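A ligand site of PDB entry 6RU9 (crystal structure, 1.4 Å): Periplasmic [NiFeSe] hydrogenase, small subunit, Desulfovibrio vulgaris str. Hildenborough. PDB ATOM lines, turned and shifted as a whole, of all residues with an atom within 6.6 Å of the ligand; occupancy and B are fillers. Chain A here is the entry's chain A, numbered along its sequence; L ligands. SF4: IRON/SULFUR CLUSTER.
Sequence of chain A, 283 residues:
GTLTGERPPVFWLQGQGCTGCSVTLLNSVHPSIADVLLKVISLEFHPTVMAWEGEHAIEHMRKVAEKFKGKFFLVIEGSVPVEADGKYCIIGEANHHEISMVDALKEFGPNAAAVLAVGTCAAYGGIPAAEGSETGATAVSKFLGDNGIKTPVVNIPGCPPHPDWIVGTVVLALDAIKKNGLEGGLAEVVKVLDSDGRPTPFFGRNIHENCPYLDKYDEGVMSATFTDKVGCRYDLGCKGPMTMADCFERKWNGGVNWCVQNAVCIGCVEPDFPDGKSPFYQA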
ATOM      1  N   ILE A 207      12.501 -18.734  -8.286  1.00  0.00           N
ATOM      2  CA  ILE A 207      11.902 -20.038  -7.968  1.00  0.00           C
ATOM      3  C   ILE A 207      10.427 -19.879  -7.629  1.00  0.00           C
ATOM      4  O   ILE A 207       9.553 -20.560  -8.175  1.00  0.00           O
ATOM      5  CB  ILE A 207      12.645 -20.679  -6.782  1.00  0.00           C
ATOM      6  CG1 ILE A 207      14.098 -21.071  -7.147  1.00  0.00           C
ATOM      7  CG2 ILE A 207      11.846 -21.855  -6.227  1.00  0.00           C
ATOM      8  CD1 ILE A 207      14.244 -22.437  -7.690  1.00  0.00           C
ATOM      9  N   HIS A 208      10.124 -18.994  -6.683  1.00  0.00           N
ATOM     10  CA  HIS A 208       8.773 -18.884  -6.138  1.00  0.00           C
ATOM     11  C   HIS A 208       7.774 -18.456  -7.193  1.00  0.00           C
ATOM     12  O   HIS A 208       6.680 -19.014  -7.275  1.00  0.00           O
ATOM     13  CB  HIS A 208       8.865 -17.878  -4.992  1.00  0.00           C
ATOM     14  CG  HIS A 208       7.554 -17.432  -4.454  1.00  0.00           C
ATOM     15  ND1 HIS A 208       6.835 -18.179  -3.555  1.00  0.00           N
ATOM     16  CD2 HIS A 208       6.823 -16.310  -4.673  1.00  0.00           C
ATOM     17  CE1 HIS A 208       5.721 -17.544  -3.235  1.00  0.00           C
ATOM     18  NE2 HIS A 208       5.682 -16.412  -3.906  1.00  0.00           N
ATOM     19  N   GLU A 209       8.123 -17.468  -8.034  1.00  0.00           N
ATOM     20  CA  GLU A 209       7.206 -16.990  -9.065  1.00  0.00           C
ATOM     21  C   GLU A 209       6.861 -18.090 -10.052  1.00  0.00           C
ATOM     22  O   GLU A 209       5.832 -18.000 -10.730  1.00  0.00           O
ATOM     23  CB  GLU A 209       7.820 -15.799  -9.778  1.00  0.00           C
ATOM     24  CG  GLU A 209       7.782 -14.558  -8.911  1.00  0.00           C
ATOM     25  CD  GLU A 209       8.560 -13.379  -9.461  1.00  0.00           C
ATOM     26  OE1 GLU A 209       9.131 -13.463 -10.578  1.00  0.00           O
ATOM     27  OE2 GLU A 209       8.613 -12.344  -8.748  1.00  0.00           O
ATOM     28  N   CYS A 211       6.806 -21.505  -9.043  1.00  0.00           N
ATOM     29  CA  CYS A 211       6.656 -22.708  -8.228  1.00  0.00           C
ATOM     30  C   CYS A 211       5.272 -23.312  -8.379  1.00  0.00           C
ATOM     31  O   CYS A 211       4.277 -22.585  -8.427  1.00  0.00           O
ATOM     32  CB  CYS A 211       6.907 -22.376  -6.752  1.00  0.00           C
ATOM     33  SG  CYS A 211       6.671 -23.771  -5.648  1.00  0.00           S
ATOM     34  N   PRO A 212       5.143 -24.647  -8.470  1.00  0.00           N
ATOM     35  CA  PRO A 212       3.789 -25.237  -8.583  1.00  0.00           C
ATOM     36  C   PRO A 212       2.912 -25.038  -7.356  1.00  0.00           C
ATOM     37  O   PRO A 212       1.681 -25.241  -7.453  1.00  0.00           O
ATOM     38  CB  PRO A 212       4.081 -26.732  -8.821  1.00  0.00           C
ATOM     39  CG  PRO A 212       5.446 -26.976  -8.314  1.00  0.00           C
ATOM     40  CD  PRO A 212       6.213 -25.660  -8.446  1.00  0.00           C
ATOM     41  N   TYR A 213       3.467 -24.646  -6.198  1.00  0.00           N
ATOM     42  CA  TYR A 213       2.662 -24.423  -4.993  1.00  0.00           C
ATOM     43  C   TYR A 213       2.314 -22.959  -4.793  1.00  0.00           C
ATOM     44  O   TYR A 213       1.776 -22.582  -3.742  1.00  0.00           O
ATOM     45  CB  TYR A 213       3.389 -25.029  -3.776  1.00  0.00           C
ATOM     46  CG  TYR A 213       3.818 -26.435  -4.046  1.00  0.00           C
ATOM     47  CD1 TYR A 213       2.888 -27.444  -4.198  1.00  0.00           C
ATOM     48  CD2 TYR A 213       5.154 -26.757  -4.218  1.00  0.00           C
ATOM     49  CE1 TYR A 213       3.286 -28.738  -4.498  1.00  0.00           C
ATOM     50  CE2 TYR A 213       5.558 -28.028  -4.525  1.00  0.00           C
ATOM     51  CZ  TYR A 213       4.624 -29.013  -4.649  1.00  0.00           C
ATOM     52  OH  TYR A 213       5.073 -30.275  -4.948  1.00  0.00           O
ATOM     53  N   LEU A 214       2.605 -22.102  -5.790  1.00  0.00           N
ATOM     54  CA  LEU A 214       2.362 -20.670  -5.654  1.00  0.00           C
ATOM     55  C   LEU A 214       0.914 -20.381  -5.275  1.00  0.00           C
ATOM     56  O   LEU A 214       0.635 -19.457  -4.499  1.00  0.00           O
ATOM     57  CB  LEU A 214       2.719 -19.975  -6.959  1.00  0.00           C
ATOM     58  CG  LEU A 214       2.576 -18.452  -6.977  1.00  0.00           C
ATOM     59  CD1 LEU A 214       3.410 -17.801  -5.874  1.00  0.00           C
ATOM     60  CD2 LEU A 214       3.003 -17.942  -8.350  1.00  0.00           C
ATOM     61  N   ASP A 215      -0.046 -21.130  -5.850  1.00  0.00           N
ATOM     62  CA  ASP A 215      -1.454 -20.898  -5.520  1.00  0.00           C
ATOM     63  C   ASP A 215      -1.696 -21.109  -4.030  1.00  0.00           C
ATOM     64  O   ASP A 215      -2.474 -20.372  -3.412  1.00  0.00           O
ATOM     65  CB  ASP A 215      -2.382 -21.783  -6.362  1.00  0.00           C
ATOM     66  CG  ASP A 215      -2.137 -23.303  -6.189  1.00  0.00           C
ATOM     67  OD1 ASP A 215      -1.028 -23.746  -5.830  1.00  0.00           O
ATOM     68  OD2 ASP A 215      -3.095 -24.068  -6.451  1.00  0.00           O
ATOM     69  N   LYS A 216      -1.040 -22.099  -3.439  1.00  0.00           N
ATOM     70  CA  LYS A 216      -1.217 -22.356  -2.014  1.00  0.00           C
ATOM     71  C   LYS A 216      -0.626 -21.230  -1.169  1.00  0.00           C
ATOM     72  O   LYS A 216      -1.218 -20.812  -0.179  1.00  0.00           O
ATOM     73  CB  LYS A 216      -0.583 -23.688  -1.646  1.00  0.00           C
ATOM     74  CG  LYS A 216      -1.112 -24.913  -2.424  1.00  0.00           C
ATOM     75  CD  LYS A 216      -2.587 -25.185  -2.146  1.00  0.00           C
ATOM     76  CE  LYS A 216      -3.061 -26.401  -2.953  1.00  0.00           C
ATOM     77  NZ  LYS A 216      -4.461 -26.729  -2.683  1.00  0.00           N
ATOM     78  N   TYR A 217       0.551 -20.723  -1.553  1.00  0.00           N
ATOM     79  CA  TYR A 217       1.103 -19.545  -0.875  1.00  0.00           C
ATOM     80  C   TYR A 217       0.133 -18.384  -0.924  1.00  0.00           C
ATOM     81  O   TYR A 217      -0.096 -17.704   0.081  1.00  0.00           O
ATOM     82  CB  TYR A 217       2.395 -19.167  -1.535  1.00  0.00           C
ATOM     83  CG  TYR A 217       3.193 -17.996  -1.031  1.00  0.00           C
ATOM     84  CD1 TYR A 217       2.952 -16.716  -1.497  1.00  0.00           C
ATOM     85  CD2 TYR A 217       4.259 -18.166  -0.159  1.00  0.00           C
ATOM     86  CE1 TYR A 217       3.751 -15.627  -1.106  1.00  0.00           C
ATOM     87  CE2 TYR A 217       5.057 -17.113   0.243  1.00  0.00           C
ATOM     88  CZ  TYR A 217       4.808 -15.844  -0.248  1.00  0.00           C
ATOM     89  OH  TYR A 217       5.609 -14.783   0.127  1.00  0.00           O
ATOM     90  N   ASP A 218      -0.408 -18.105  -2.113  1.00  0.00           N
ATOM     91  CA  ASP A 218      -1.296 -16.954  -2.252  1.00  0.00           C
ATOM     92  C   ASP A 218      -2.580 -17.141  -1.460  1.00  0.00           C
ATOM     93  O   ASP A 218      -3.187 -16.162  -1.011  1.00  0.00           O
ATOM     94  CB  ASP A 218      -1.603 -16.729  -3.727  1.00  0.00           C
ATOM     95  CG  ASP A 218      -0.406 -16.217  -4.507  1.00  0.00           C
ATOM     96  OD1 ASP A 218       0.562 -15.691  -3.907  1.00  0.00           O
ATOM     97  OD2 ASP A 218      -0.446 -16.342  -5.765  1.00  0.00           O
ATOM     98  N   MET A 222      -0.544 -23.666   4.158  1.00  0.00           N
ATOM     99  CA  MET A 222       0.827 -24.022   4.476  1.00  0.00           C
ATOM    100  C   MET A 222       0.896 -25.420   5.088  1.00  0.00           C
ATOM    101  O   MET A 222       0.149 -25.736   6.029  1.00  0.00           O
ATOM    102  CB  MET A 222       1.416 -23.028   5.468  1.00  0.00           C
ATOM    103  CG  MET A 222       1.447 -21.610   4.963  1.00  0.00           C
ATOM    104  SD  MET A 222       2.609 -21.503   3.629  1.00  0.00           S
ATOM    105  CE  MET A 222       2.305 -19.810   3.086  1.00  0.00           C
ATOM    106  N   GLY A 231       0.391 -28.481   0.655  1.00  0.00           N
ATOM    107  CA  GLY A 231       0.520 -27.066   0.969  1.00  0.00           C
ATOM    108  C   GLY A 231       1.854 -26.488   0.528  1.00  0.00           C
ATOM    109  O   GLY A 231       2.798 -27.199   0.188  1.00  0.00           O
ATOM    110  N   CYS A 232       1.918 -25.162   0.556  1.00  0.00           N
ATOM    111  CA  CYS A 232       3.172 -24.429   0.389  1.00  0.00           C
ATOM    112  C   CYS A 232       4.109 -24.729   1.550  1.00  0.00           C
ATOM    113  O   CYS A 232       3.682 -24.967   2.677  1.00  0.00           O
ATOM    114  CB  CYS A 232       2.860 -22.935   0.305  1.00  0.00           C
ATOM    115  SG  CYS A 232       4.248 -21.801   0.435  1.00  0.00           S
ATOM    116  N   ARG A 233       5.417 -24.686   1.259  1.00  0.00           N
ATOM    117  CA  ARG A 233       6.488 -24.983   2.191  1.00  0.00           C
ATOM    118  C   ARG A 233       7.036 -23.775   2.944  1.00  0.00           C
ATOM    119  O   ARG A 233       8.012 -23.915   3.712  1.00  0.00           O
ATOM    120  CB  ARG A 233       7.625 -25.694   1.459  1.00  0.00           C
ATOM    121  CG  ARG A 233       7.320 -27.134   1.073  1.00  0.00           C
ATOM    122  CD  ARG A 233       6.278 -27.267  -0.072  1.00  0.00           C
ATOM    123  NE  ARG A 233       6.499 -28.556  -0.739  1.00  0.00           N
ATOM    124  CZ  ARG A 233       5.583 -29.333  -1.326  1.00  0.00           C
ATOM    125  NH1 ARG A 233       4.299 -28.986  -1.370  1.00  0.00           N
ATOM    126  NH2 ARG A 233       5.956 -30.497  -1.849  1.00  0.00           N
ATOM    127  N   TYR A 234       6.420 -22.611   2.788  1.00  0.00           N
ATOM    128  CA  TYR A 234       6.980 -21.384   3.370  1.00  0.00           C
ATOM    129  C   TYR A 234       7.138 -21.491   4.877  1.00  0.00           C
ATOM    130  O   TYR A 234       8.182 -21.117   5.433  1.00  0.00           O
ATOM    131  CB  TYR A 234       6.087 -20.204   3.009  1.00  0.00           C
ATOM    132  CG  TYR A 234       6.539 -18.879   3.592  1.00  0.00           C
ATOM    133  CD1 TYR A 234       7.438 -18.059   2.914  1.00  0.00           C
ATOM    134  CD2 TYR A 234       6.049 -18.413   4.801  1.00  0.00           C
ATOM    135  CE1 TYR A 234       7.843 -16.828   3.420  1.00  0.00           C
ATOM    136  CE2 TYR A 234       6.428 -17.167   5.309  1.00  0.00           C
ATOM    137  CZ  TYR A 234       7.331 -16.396   4.616  1.00  0.00           C
ATOM    138  OH  TYR A 234       7.748 -15.183   5.104  1.00  0.00           O
ATOM    139  N   ASP A 235       6.107 -21.991   5.576  1.00  0.00           N
ATOM    140  CA  ASP A 235       6.215 -22.038   7.028  1.00  0.00           C
ATOM    141  C   ASP A 235       7.264 -23.050   7.494  1.00  0.00           C
ATOM    142  O   ASP A 235       7.795 -22.906   8.606  1.00  0.00           O
ATOM    143  CB  ASP A 235       4.873 -22.388   7.662  1.00  0.00           C
ATOM    144  CG  ASP A 235       3.865 -21.228   7.644  1.00  0.00           C
ATOM    145  OD1 ASP A 235       4.214 -20.079   7.267  1.00  0.00           O
ATOM    146  OD2 ASP A 235       2.701 -21.482   8.029  1.00  0.00           O
ATOM    147  N   CYS A 238      10.872 -22.615   3.429  1.00  0.00           N
ATOM    148  CA  CYS A 238      11.231 -22.484   2.010  1.00  0.00           C
ATOM    149  C   CYS A 238      11.701 -21.071   1.703  1.00  0.00           C
ATOM    150  O   CYS A 238      11.004 -20.103   2.013  1.00  0.00           O
ATOM    151  CB  CYS A 238      10.027 -22.795   1.128  1.00  0.00           C
ATOM    152  SG  CYS A 238      10.484 -22.846  -0.622  1.00  0.00           S
ATOM    153  N   LYS A 239      12.883 -20.949   1.080  1.00  0.00           N
ATOM    154  CA  LYS A 239      13.458 -19.669   0.685  1.00  0.00           C
ATOM    155  C   LYS A 239      13.252 -19.354  -0.803  1.00  0.00           C
ATOM    156  O   LYS A 239      13.906 -18.467  -1.363  1.00  0.00           O
ATOM    157  CB  LYS A 239      14.931 -19.584   1.094  1.00  0.00           C
ATOM    158  CG  LYS A 239      15.205 -19.888   2.571  1.00  0.00           C
ATOM    159  CD  LYS A 239      14.316 -19.067   3.498  1.00  0.00           C
ATOM    160  CE  LYS A 239      14.743 -19.145   4.970  1.00  0.00           C
ATOM    161  NZ  LYS A 239      14.839 -20.551   5.456  1.00  0.00           N
ATOM    162  N   GLY A 240      12.343 -20.085  -1.471  1.00  0.00           N
ATOM    163  CA  GLY A 240      12.054 -19.827  -2.859  1.00  0.00           C
ATOM    164  C   GLY A 240      11.758 -18.375  -3.191  1.00  0.00           C
ATOM    165  O   GLY A 240      12.172 -17.887  -4.253  1.00  0.00           O
ATOM    166  N   PRO A 241      11.038 -17.647  -2.316  1.00  0.00           N
ATOM    167  CA  PRO A 241      10.755 -16.233  -2.636  1.00  0.00           C
ATOM    168  C   PRO A 241      11.989 -15.374  -2.850  1.00  0.00           C
ATOM    169  O   PRO A 241      11.887 -14.319  -3.506  1.00  0.00           O
ATOM    170  CB  PRO A 241       9.923 -15.743  -1.444  1.00  0.00           C
ATOM    171  CG  PRO A 241       9.278 -17.020  -0.945  1.00  0.00           C
ATOM    172  CD  PRO A 241      10.353 -18.077  -1.090  1.00  0.00           C
ATOM    173  N   TRP A 258      13.228 -32.474  -6.802  1.00  0.00           N
ATOM    174  CA  TRP A 258      13.872 -31.199  -6.523  1.00  0.00           C
ATOM    175  C   TRP A 258      13.529 -30.776  -5.109  1.00  0.00           C
ATOM    176  O   TRP A 258      12.655 -31.329  -4.445  1.00  0.00           O
ATOM    177  CB  TRP A 258      13.521 -30.095  -7.505  1.00  0.00           C
ATOM    178  CG  TRP A 258      12.127 -29.586  -7.514  1.00  0.00           C
ATOM    179  CD1 TRP A 258      10.974 -30.310  -7.741  1.00  0.00           C
ATOM    180  CD2 TRP A 258      11.722 -28.223  -7.358  1.00  0.00           C
ATOM    181  NE1 TRP A 258       9.881 -29.460  -7.740  1.00  0.00           N
ATOM    182  CE2 TRP A 258      10.317 -28.181  -7.506  1.00  0.00           C
ATOM    183  CE3 TRP A 258      12.408 -27.028  -7.126  1.00  0.00           C
ATOM    184  CZ2 TRP A 258       9.586 -26.989  -7.408  1.00  0.00           C
ATOM    185  CZ3 TRP A 258      11.672 -25.832  -7.035  1.00  0.00           C
ATOM    186  CH2 TRP A 258      10.286 -25.828  -7.178  1.00  0.00           C
ATOM    187  N   VAL A 260      12.141 -28.307  -3.448  1.00  0.00           N
ATOM    188  CA  VAL A 260      10.831 -27.832  -2.968  1.00  0.00           C
ATOM    189  C   VAL A 260       9.848 -28.997  -2.898  1.00  0.00           C
ATOM    190  O   VAL A 260       9.055 -29.092  -1.948  1.00  0.00           O
ATOM    191  CB  VAL A 260      10.323 -26.666  -3.839  1.00  0.00           C
ATOM    192  CG1 VAL A 260       8.894 -26.301  -3.508  1.00  0.00           C
ATOM    193  CG2 VAL A 260      11.213 -25.444  -3.658  1.00  0.00           C
ATOM    194  N   ALA A 263      11.399 -31.256   0.173  1.00  0.00           N
ATOM    195  CA  ALA A 263      11.575 -30.616   1.472  1.00  0.00           C
ATOM    196  C   ALA A 263      11.338 -29.122   1.308  1.00  0.00           C
ATOM    197  O   ALA A 263      10.194 -28.694   1.155  1.00  0.00           O
ATOM    198  CB  ALA A 263      12.953 -30.983   2.018  1.00  0.00           C
ATOM    199  N   CYS A 265      13.358 -25.301  -0.352  1.00  0.00           N
ATOM    200  CA  CYS A 265      14.518 -24.621  -0.931  1.00  0.00           C
ATOM    201  C   CYS A 265      15.283 -23.892   0.173  1.00  0.00           C
ATOM    202  O   CYS A 265      14.674 -23.195   1.007  1.00  0.00           O
ATOM    203  CB  CYS A 265      14.057 -23.608  -1.989  1.00  0.00           C
ATOM    204  SG  CYS A 265      15.342 -22.574  -2.754  1.00  0.00           S
HETATM  205 FE1  SF4 L   1       8.483 -22.174  -1.580  1.00  0.00          FE
HETATM  206 FE2  SF4 L   1       7.136 -20.132  -2.799  1.00  0.00          FE
HETATM  207 FE3  SF4 L   1       5.716 -21.893  -1.279  1.00  0.00          FE
HETATM  208 FE4  SF4 L   1       6.832 -22.635  -3.677  1.00  0.00          FE
HETATM  209  S1  SF4 L   1       5.095 -21.131  -3.357  1.00  0.00           S
HETATM  210  S2  SF4 L   1       6.849 -23.854  -1.714  1.00  0.00           S
HETATM  211  S3  SF4 L   1       8.809 -21.402  -3.710  1.00  0.00           S
HETATM  212  S4  SF4 L   1       7.385 -20.445  -0.541  1.00  0.00           S
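The backbone NH (N) of His 208 sits at hydrogen-bond distance from the backbone carbonyl oxygen (O) of Gly 240 (3.4 Å).
The side-chain sulfur (SG) of Cys 238 lies close to the backbone NH (N) of Cys 265 (3.8 Å).
N of Tyr 213 lies close to SG of Cys 211, 3.4 Å away.
The backbone NH (N) of Gly 240 lies close to the side-chain sulfur (SG) of Cys 238, at 3.4 Å.
The backbone carbonyl oxygen (O) of Val 260 sits at hydrogen-bond distance from the guanidinium group (NE) of Arg 233 (2.9 Å).
SG of Cys 232 sits close to SD of Met 222 (3.6 Å).
The guanidinium group of Arg 233 is in hydrogen-bond range of the backbone carbonyl oxygen of Gly 231 (2.8 Å).
The backbone carbonyl oxygen (O) of Arg 233 is in hydrogen-bond range of the backbone NH (N) of Cys 238 (3.2 Å).
S1 of the ligand lies close to O of Tyr 213 (3.6 Å).
Ile 207 touches the ligand (CG2 to S3, 3.97 Å).
Tyr 217 touches the ligand.
Tyr 234 touches the ligand.
CA of Gly 240 touches S3 of the ligand (3.7 Å).
Pro 241 touches the ligand.
CG1 of Val 260 touches S2 of the ligand, at 3.7 Å.
A sulfur (S1) of the ligand lies close to the backbone NH (N) of Leu 214.
The backbone NH of Arg 233 lies close to a sulfur (S2) of the ligand (3.4 Å).
An iron atom (FE2) of the ligand is bound by a ring nitrogen (ND1) of His 208, at 2.1 Å.
An iron atom (FE4) of the ligand is bound by the side-chain sulfur (SG) of Cys 211 (2.3 Å).
The side-chain sulfur (SG) of Cys 232 is bound to an iron atom (FE3) of the ligand, at 2.3 Å.
SG of Cys 238 binds FE1 of the ligand (2.3 Å).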
